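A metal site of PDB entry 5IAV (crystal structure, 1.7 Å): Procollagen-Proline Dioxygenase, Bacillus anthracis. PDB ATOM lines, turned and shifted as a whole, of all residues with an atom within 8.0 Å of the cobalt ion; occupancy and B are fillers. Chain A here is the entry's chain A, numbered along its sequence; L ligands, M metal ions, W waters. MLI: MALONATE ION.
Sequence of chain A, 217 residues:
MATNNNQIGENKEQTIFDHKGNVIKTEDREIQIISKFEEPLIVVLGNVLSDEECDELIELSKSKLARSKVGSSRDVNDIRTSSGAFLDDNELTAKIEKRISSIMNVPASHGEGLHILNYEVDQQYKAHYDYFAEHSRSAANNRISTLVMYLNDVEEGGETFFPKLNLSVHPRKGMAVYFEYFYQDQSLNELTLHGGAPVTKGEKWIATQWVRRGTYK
The cobalt ion is bound by OD1 of Asp 130 (2.1 Å), NE2 of His 128 (2.1 Å), NE2 of His 194 (2.1 Å), water W2 (2.1 Å) and water W1 (2.4 Å).
Slightly farther from the cobalt ion lies an oxygen (O6) of the ligand (2.6 Å).
The side-chain carboxylate (OD2) of Asp 130 sits at hydrogen-bond distance from the indole nitrogen (NE1) of Trp 210 (3.1 Å).
The side-chain carboxylate of Asp 130 lies within hydrogen-bond range of the side-chain hydroxyl of Thr 146 (2.6 Å).
The guanidinium group of Arg 143 is in hydrogen-bond range of the backbone carbonyl oxygen of Asp 130.
O of Lys 126 lies within hydrogen-bond range of ND1 of His 128 (2.8 Å).
The backbone carbonyl oxygen of Thr 192 is in hydrogen-bond range of a ring nitrogen (ND1) of His 194, 2.8 Å away.
Of the 22 residues printed, 3 come within 4 Å of the cobalt ion.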
ATOM      1  N   TYR A 125      -6.702  14.879  -0.601  1.00  0.00           N
ATOM      2  CA  TYR A 125      -7.856  14.379  -1.306  1.00  0.00           C
ATOM      3  C   TYR A 125      -7.321  13.603  -2.475  1.00  0.00           C
ATOM      4  O   TYR A 125      -6.717  14.134  -3.359  1.00  0.00           O
ATOM      5  CB  TYR A 125      -8.693  15.537  -1.775  1.00  0.00           C
ATOM      6  CG  TYR A 125     -10.119  15.335  -1.595  1.00  0.00           C
ATOM      7  CD1 TYR A 125     -10.703  15.442  -0.350  1.00  0.00           C
ATOM      8  CD2 TYR A 125     -10.902  15.029  -2.668  1.00  0.00           C
ATOM      9  CE1 TYR A 125     -12.068  15.244  -0.194  1.00  0.00           C
ATOM     10  CE2 TYR A 125     -12.243  14.836  -2.538  1.00  0.00           C
ATOM     11  CZ  TYR A 125     -12.812  14.949  -1.308  1.00  0.00           C
ATOM     12  OH  TYR A 125     -14.150  14.749  -1.249  1.00  0.00           O
ATOM     13  N   LYS A 126      -7.580  12.311  -2.467  1.00  0.00           N
ATOM     14  CA  LYS A 126      -7.000  11.417  -3.463  1.00  0.00           C
ATOM     15  C   LYS A 126      -7.523  11.726  -4.866  1.00  0.00           C
ATOM     16  O   LYS A 126      -8.672  12.139  -5.039  1.00  0.00           O
ATOM     17  CB  LYS A 126      -7.303   9.962  -3.096  1.00  0.00           C
ATOM     18  CG  LYS A 126      -6.693   9.506  -1.787  1.00  0.00           C
ATOM     19  CD  LYS A 126      -5.195   9.722  -1.790  1.00  0.00           C
ATOM     20  N   ALA A 127      -6.678  11.475  -5.869  1.00  0.00           N
ATOM     21  CA  ALA A 127      -7.045  11.818  -7.237  1.00  0.00           C
ATOM     22  C   ALA A 127      -8.282  11.051  -7.690  1.00  0.00           C
ATOM     23  O   ALA A 127      -8.461   9.865  -7.367  1.00  0.00           O
ATOM     24  CB  ALA A 127      -5.886  11.543  -8.191  1.00  0.00           C
ATOM     25  N   HIS A 128      -9.118  11.730  -8.484  1.00  0.00           N
ATOM     26  CA  HIS A 128     -10.415  11.189  -8.892  1.00  0.00           C
ATOM     27  C   HIS A 128     -10.922  11.975 -10.101  1.00  0.00           C
ATOM     28  O   HIS A 128     -10.357  12.995 -10.481  1.00  0.00           O
ATOM     29  CB  HIS A 128     -11.444  11.314  -7.766  1.00  0.00           C
ATOM     30  CG  HIS A 128     -11.647  12.732  -7.355  1.00  0.00           C
ATOM     31  ND1 HIS A 128     -10.762  13.378  -6.514  1.00  0.00           N
ATOM     32  CD2 HIS A 128     -12.551  13.670  -7.746  1.00  0.00           C
ATOM     33  CE1 HIS A 128     -11.146  14.641  -6.361  1.00  0.00           C
ATOM     34  NE2 HIS A 128     -12.201  14.853  -7.122  1.00  0.00           N
ATOM     35  N   TYR A 129     -12.019  11.474 -10.667  1.00  0.00           N
ATOM     36  CA  TYR A 129     -12.801  12.181 -11.675  1.00  0.00           C
ATOM     37  C   TYR A 129     -14.012  12.807 -11.006  1.00  0.00           C
ATOM     38  O   TYR A 129     -14.587  12.235 -10.076  1.00  0.00           O
ATOM     39  CB  TYR A 129     -13.254  11.231 -12.792  1.00  0.00           C
ATOM     40  CG  TYR A 129     -12.073  10.540 -13.418  1.00  0.00           C
ATOM     41  CD1 TYR A 129     -11.295  11.187 -14.369  1.00  0.00           C
ATOM     42  CD2 TYR A 129     -11.668   9.269 -12.976  1.00  0.00           C
ATOM     43  CE1 TYR A 129     -10.184  10.598 -14.921  1.00  0.00           C
ATOM     44  CE2 TYR A 129     -10.530   8.668 -13.533  1.00  0.00           C
ATOM     45  CZ  TYR A 129      -9.804   9.341 -14.491  1.00  0.00           C
ATOM     46  OH  TYR A 129      -8.682   8.774 -15.064  1.00  0.00           O
ATOM     47  N   ASP A 130     -14.418  13.995 -11.480  1.00  0.00           N
ATOM     48  CA  ASP A 130     -15.636  14.540 -10.912  1.00  0.00           C
ATOM     49  C   ASP A 130     -16.867  13.956 -11.574  1.00  0.00           C
ATOM     50  O   ASP A 130     -17.922  13.948 -10.947  1.00  0.00           O
ATOM     51  CB  ASP A 130     -15.666  16.083 -11.027  1.00  0.00           C
ATOM     52  CG  ASP A 130     -14.862  16.767  -9.916  1.00  0.00           C
ATOM     53  OD1 ASP A 130     -14.321  16.081  -8.997  1.00  0.00           O
ATOM     54  OD2 ASP A 130     -14.766  18.018  -9.954  1.00  0.00           O
ATOM     55  N   TYR A 131     -16.757  13.502 -12.820  1.00  0.00           N
ATOM     56  CA  TYR A 131     -17.927  12.943 -13.497  1.00  0.00           C
ATOM     57  C   TYR A 131     -18.096  11.477 -13.102  1.00  0.00           C
ATOM     58  O   TYR A 131     -17.203  10.848 -12.530  1.00  0.00           O
ATOM     59  CB  TYR A 131     -17.811  13.059 -15.013  1.00  0.00           C
ATOM     60  CG  TYR A 131     -16.565  12.461 -15.618  1.00  0.00           C
ATOM     61  CD1 TYR A 131     -15.396  13.218 -15.760  1.00  0.00           C
ATOM     62  CD2 TYR A 131     -16.545  11.136 -16.048  1.00  0.00           C
ATOM     63  CE1 TYR A 131     -14.250  12.666 -16.323  1.00  0.00           C
ATOM     64  CE2 TYR A 131     -15.413  10.581 -16.612  1.00  0.00           C
ATOM     65  CZ  TYR A 131     -14.263  11.348 -16.744  1.00  0.00           C
ATOM     66  OH  TYR A 131     -13.133  10.801 -17.319  1.00  0.00           O
ATOM     67  N   ARG A 143     -22.291  15.033 -14.458  1.00  0.00           N
ATOM     68  CA  ARG A 143     -21.554  16.291 -14.328  1.00  0.00           C
ATOM     69  C   ARG A 143     -20.763  16.555 -15.582  1.00  0.00           C
ATOM     70  O   ARG A 143     -20.242  15.639 -16.213  1.00  0.00           O
ATOM     71  CB  ARG A 143     -20.622  16.227 -13.109  1.00  0.00           C
ATOM     72  CG  ARG A 143     -21.335  16.194 -11.796  1.00  0.00           C
ATOM     73  CD  ARG A 143     -20.356  15.857 -10.705  1.00  0.00           C
ATOM     74  NE  ARG A 143     -20.953  15.876  -9.364  1.00  0.00           N
ATOM     75  CZ  ARG A 143     -20.327  15.407  -8.288  1.00  0.00           C
ATOM     76  NH1 ARG A 143     -19.102  14.900  -8.385  1.00  0.00           N
ATOM     77  NH2 ARG A 143     -20.906  15.498  -7.102  1.00  0.00           N
ATOM     78  N   THR A 146     -16.683  21.794 -13.438  1.00  0.00           N
ATOM     79  CA  THR A 146     -16.436  22.020 -12.032  1.00  0.00           C
ATOM     80  C   THR A 146     -15.840  23.406 -11.861  1.00  0.00           C
ATOM     81  O   THR A 146     -15.001  23.816 -12.655  1.00  0.00           O
ATOM     82  CB  THR A 146     -15.415  20.998 -11.458  1.00  0.00           C
ATOM     83  OG1 THR A 146     -16.006  19.690 -11.492  1.00  0.00           O
ATOM     84  CG2 THR A 146     -15.013  21.319 -10.039  1.00  0.00           C
ATOM     85  N   VAL A 148     -13.801  25.147  -8.603  1.00  0.00           N
ATOM     86  CA  VAL A 148     -13.256  25.029  -7.250  1.00  0.00           C
ATOM     87  C   VAL A 148     -12.767  26.393  -6.817  1.00  0.00           C
ATOM     88  O   VAL A 148     -11.872  26.979  -7.467  1.00  0.00           O
ATOM     89  CB  VAL A 148     -12.122  24.004  -7.179  1.00  0.00           C
ATOM     90  CG1 VAL A 148     -11.399  24.079  -5.820  1.00  0.00           C
ATOM     91  CG2 VAL A 148     -12.653  22.604  -7.479  1.00  0.00           C
ATOM     92  N   THR A 160      -4.336  21.987  -6.069  1.00  0.00           N
ATOM     93  CA  THR A 160      -5.223  21.171  -6.891  1.00  0.00           C
ATOM     94  C   THR A 160      -4.352  20.698  -8.042  1.00  0.00           C
ATOM     95  O   THR A 160      -3.855  21.519  -8.832  1.00  0.00           O
ATOM     96  CB  THR A 160      -6.402  22.000  -7.446  1.00  0.00           C
ATOM     97  OG1 THR A 160      -7.164  22.633  -6.380  1.00  0.00           O
ATOM     98  CG2 THR A 160      -7.349  21.098  -8.294  1.00  0.00           C
ATOM     99  N   PHE A 162      -3.310  18.043 -11.358  1.00  0.00           N
ATOM    100  CA  PHE A 162      -3.806  17.255 -12.475  1.00  0.00           C
ATOM    101  C   PHE A 162      -2.687  16.309 -12.915  1.00  0.00           C
ATOM    102  O   PHE A 162      -1.869  16.686 -13.761  1.00  0.00           O
ATOM    103  CB  PHE A 162      -4.244  18.157 -13.626  1.00  0.00           C
ATOM    104  CG  PHE A 162      -5.447  19.011 -13.295  1.00  0.00           C
ATOM    105  CD1 PHE A 162      -5.318  20.206 -12.596  1.00  0.00           C
ATOM    106  CD2 PHE A 162      -6.718  18.593 -13.670  1.00  0.00           C
ATOM    107  CE1 PHE A 162      -6.441  20.969 -12.267  1.00  0.00           C
ATOM    108  CE2 PHE A 162      -7.846  19.330 -13.361  1.00  0.00           C
ATOM    109  CZ  PHE A 162      -7.734  20.505 -12.649  1.00  0.00           C
ATOM    110  N   PHE A 179     -12.719  23.747 -14.624  1.00  0.00           N
ATOM    111  CA  PHE A 179     -12.332  22.791 -15.655  1.00  0.00           C
ATOM    112  C   PHE A 179     -13.563  22.071 -16.144  1.00  0.00           C
ATOM    113  O   PHE A 179     -14.551  21.949 -15.417  1.00  0.00           O
ATOM    114  CB  PHE A 179     -11.265  21.778 -15.181  1.00  0.00           C
ATOM    115  CG  PHE A 179     -11.582  21.068 -13.875  1.00  0.00           C
ATOM    116  CD1 PHE A 179     -11.330  21.685 -12.645  1.00  0.00           C
ATOM    117  CD2 PHE A 179     -12.006  19.753 -13.854  1.00  0.00           C
ATOM    118  CE1 PHE A 179     -11.565  21.013 -11.439  1.00  0.00           C
ATOM    119  CE2 PHE A 179     -12.215  19.066 -12.635  1.00  0.00           C
ATOM    120  CZ  PHE A 179     -12.021  19.714 -11.437  1.00  0.00           C
ATOM    121  N   TYR A 181     -15.174  18.666 -18.640  1.00  0.00           N
ATOM    122  CA  TYR A 181     -14.988  17.313 -19.134  1.00  0.00           C
ATOM    123  C   TYR A 181     -16.259  16.843 -19.817  1.00  0.00           C
ATOM    124  O   TYR A 181     -16.885  15.881 -19.390  1.00  0.00           O
ATOM    125  CB  TYR A 181     -14.662  16.414 -17.928  1.00  0.00           C
ATOM    126  CG  TYR A 181     -15.364  16.842 -16.645  1.00  0.00           C
ATOM    127  CD1 TYR A 181     -16.627  16.379 -16.343  1.00  0.00           C
ATOM    128  CD2 TYR A 181     -14.776  17.740 -15.771  1.00  0.00           C
ATOM    129  CE1 TYR A 181     -17.271  16.765 -15.192  1.00  0.00           C
ATOM    130  CE2 TYR A 181     -15.409  18.137 -14.613  1.00  0.00           C
ATOM    131  CZ  TYR A 181     -16.671  17.655 -14.335  1.00  0.00           C
ATOM    132  OH  TYR A 181     -17.333  18.032 -13.199  1.00  0.00           O
ATOM    133  N   THR A 192      -8.772  15.063 -17.062  1.00  0.00           N
ATOM    134  CA  THR A 192      -9.082  15.925 -15.935  1.00  0.00           C
ATOM    135  C   THR A 192      -9.003  15.218 -14.587  1.00  0.00           C
ATOM    136  O   THR A 192      -9.429  15.777 -13.581  1.00  0.00           O
ATOM    137  CB  THR A 192     -10.476  16.573 -16.095  1.00  0.00           C
ATOM    138  OG1 THR A 192     -11.491  15.576 -15.939  1.00  0.00           O
ATOM    139  CG2 THR A 192     -10.597  17.287 -17.422  1.00  0.00           C
ATOM    140  N   LEU A 193      -8.461  13.991 -14.530  1.00  0.00           N
ATOM    141  CA  LEU A 193      -8.133  13.396 -13.243  1.00  0.00           C
ATOM    142  C   LEU A 193      -7.447  14.432 -12.370  1.00  0.00           C
ATOM    143  O   LEU A 193      -6.587  15.167 -12.856  1.00  0.00           O
ATOM    144  CB  LEU A 193      -7.207  12.189 -13.458  1.00  0.00           C
ATOM    145  CG  LEU A 193      -6.744  11.511 -12.155  1.00  0.00           C
ATOM    146  CD1 LEU A 193      -7.905  10.710 -11.591  1.00  0.00           C
ATOM    147  CD2 LEU A 193      -5.529  10.628 -12.447  1.00  0.00           C
ATOM    148  N   HIS A 194      -7.887  14.580 -11.119  1.00  0.00           N
ATOM    149  CA  HIS A 194      -7.305  15.628 -10.278  1.00  0.00           C
ATOM    150  C   HIS A 194      -7.449  15.241  -8.815  1.00  0.00           C
ATOM    151  O   HIS A 194      -8.302  14.431  -8.445  1.00  0.00           O
ATOM    152  CB  HIS A 194      -7.971  16.981 -10.491  1.00  0.00           C
ATOM    153  CG  HIS A 194      -9.411  16.953 -10.151  1.00  0.00           C
ATOM    154  ND1 HIS A 194     -10.350  16.414 -10.998  1.00  0.00           N
ATOM    155  CD2 HIS A 194     -10.069  17.271  -9.008  1.00  0.00           C
ATOM    156  CE1 HIS A 194     -11.534  16.424 -10.403  1.00  0.00           C
ATOM    157  NE2 HIS A 194     -11.391  16.943  -9.193  1.00  0.00           N
ATOM    158  N   GLY A 195      -6.593  15.835  -7.976  1.00  0.00           N
ATOM    159  CA  GLY A 195      -6.698  15.648  -6.547  1.00  0.00           C
ATOM    160  C   GLY A 195      -6.368  16.923  -5.800  1.00  0.00           C
ATOM    161  O   GLY A 195      -6.077  17.970  -6.388  1.00  0.00           O
ATOM    162  N   GLY A 196      -6.501  16.820  -4.482  1.00  0.00           N
ATOM    163  CA  GLY A 196      -6.062  17.880  -3.594  1.00  0.00           C
ATOM    164  C   GLY A 196      -4.807  17.426  -2.892  1.00  0.00           C
ATOM    165  O   GLY A 196      -4.828  16.433  -2.157  1.00  0.00           O
ATOM    166  N   ILE A 206     -12.282  24.871   0.660  1.00  0.00           N
ATOM    167  CA  ILE A 206     -12.737  25.160  -0.703  1.00  0.00           C
ATOM    168  C   ILE A 206     -14.253  25.070  -0.807  1.00  0.00           C
ATOM    169  O   ILE A 206     -14.904  24.300  -0.101  1.00  0.00           O
ATOM    170  CB  ILE A 206     -12.133  24.251  -1.798  1.00  0.00           C
ATOM    171  CG1 ILE A 206     -12.395  22.777  -1.470  1.00  0.00           C
ATOM    172  CG2 ILE A 206     -10.632  24.482  -1.927  1.00  0.00           C
ATOM    173  CD1 ILE A 206     -12.003  21.836  -2.581  1.00  0.00           C
ATOM    174  N   THR A 208     -17.023  24.143  -3.911  1.00  0.00           N
ATOM    175  CA  THR A 208     -17.097  23.573  -5.254  1.00  0.00           C
ATOM    176  C   THR A 208     -18.498  23.660  -5.778  1.00  0.00           C
ATOM    177  O   THR A 208     -19.446  23.320  -5.069  1.00  0.00           O
ATOM    178  CB  THR A 208     -16.680  22.105  -5.266  1.00  0.00           C
ATOM    179  OG1 THR A 208     -15.420  21.981  -4.653  1.00  0.00           O
ATOM    180  CG2 THR A 208     -16.593  21.554  -6.698  1.00  0.00           C
ATOM    181  N   TRP A 210     -20.392  21.805  -8.836  1.00  0.00           N
ATOM    182  CA  TRP A 210     -20.479  20.804  -9.896  1.00  0.00           C
ATOM    183  C   TRP A 210     -21.713  21.103 -10.746  1.00  0.00           C
ATOM    184  O   TRP A 210     -22.800  21.353 -10.207  1.00  0.00           O
ATOM    185  CB  TRP A 210     -20.575  19.375  -9.333  1.00  0.00           C
ATOM    186  CG  TRP A 210     -19.327  18.964  -8.557  1.00  0.00           C
ATOM    187  CD1 TRP A 210     -18.054  18.781  -9.085  1.00  0.00           C
ATOM    188  CD2 TRP A 210     -19.201  18.735  -7.147  1.00  0.00           C
ATOM    189  NE1 TRP A 210     -17.190  18.425  -8.105  1.00  0.00           N
ATOM    190  CE2 TRP A 210     -17.847  18.400  -6.902  1.00  0.00           C
ATOM    191  CE3 TRP A 210     -20.107  18.743  -6.069  1.00  0.00           C
ATOM    192  CZ2 TRP A 210     -17.357  18.106  -5.629  1.00  0.00           C
ATOM    193  CZ3 TRP A 210     -19.614  18.463  -4.794  1.00  0.00           C
ATOM    194  CH2 TRP A 210     -18.253  18.145  -4.581  1.00  0.00           C
HETATM  195  C1  MLI L   1      -9.811  19.646  -5.440  1.00  0.00           C
HETATM  196  C2  MLI L   1     -10.218  18.192  -5.205  1.00  0.00           C
HETATM  197  C3  MLI L   1      -8.939  20.258  -4.342  1.00  0.00           C
HETATM  198  O6  MLI L   1     -10.945  17.624  -6.140  1.00  0.00           O
HETATM  199  O7  MLI L   1      -9.940  17.576  -4.139  1.00  0.00           O
HETATM  200  O8  MLI L   1      -8.158  21.220  -4.569  1.00  0.00           O
HETATM  201  O9  MLI L   1      -9.072  19.800  -3.111  1.00  0.00           O
HETATM  202 CO    CO M   1     -12.841  16.726  -7.713  1.00  0.00          CO
HETATM  203  O   HOH W   1     -14.162  16.575  -5.673  1.00  0.00           O
HETATM  204  O   HOH W   2     -13.391  18.737  -7.479  1.00  0.00           O
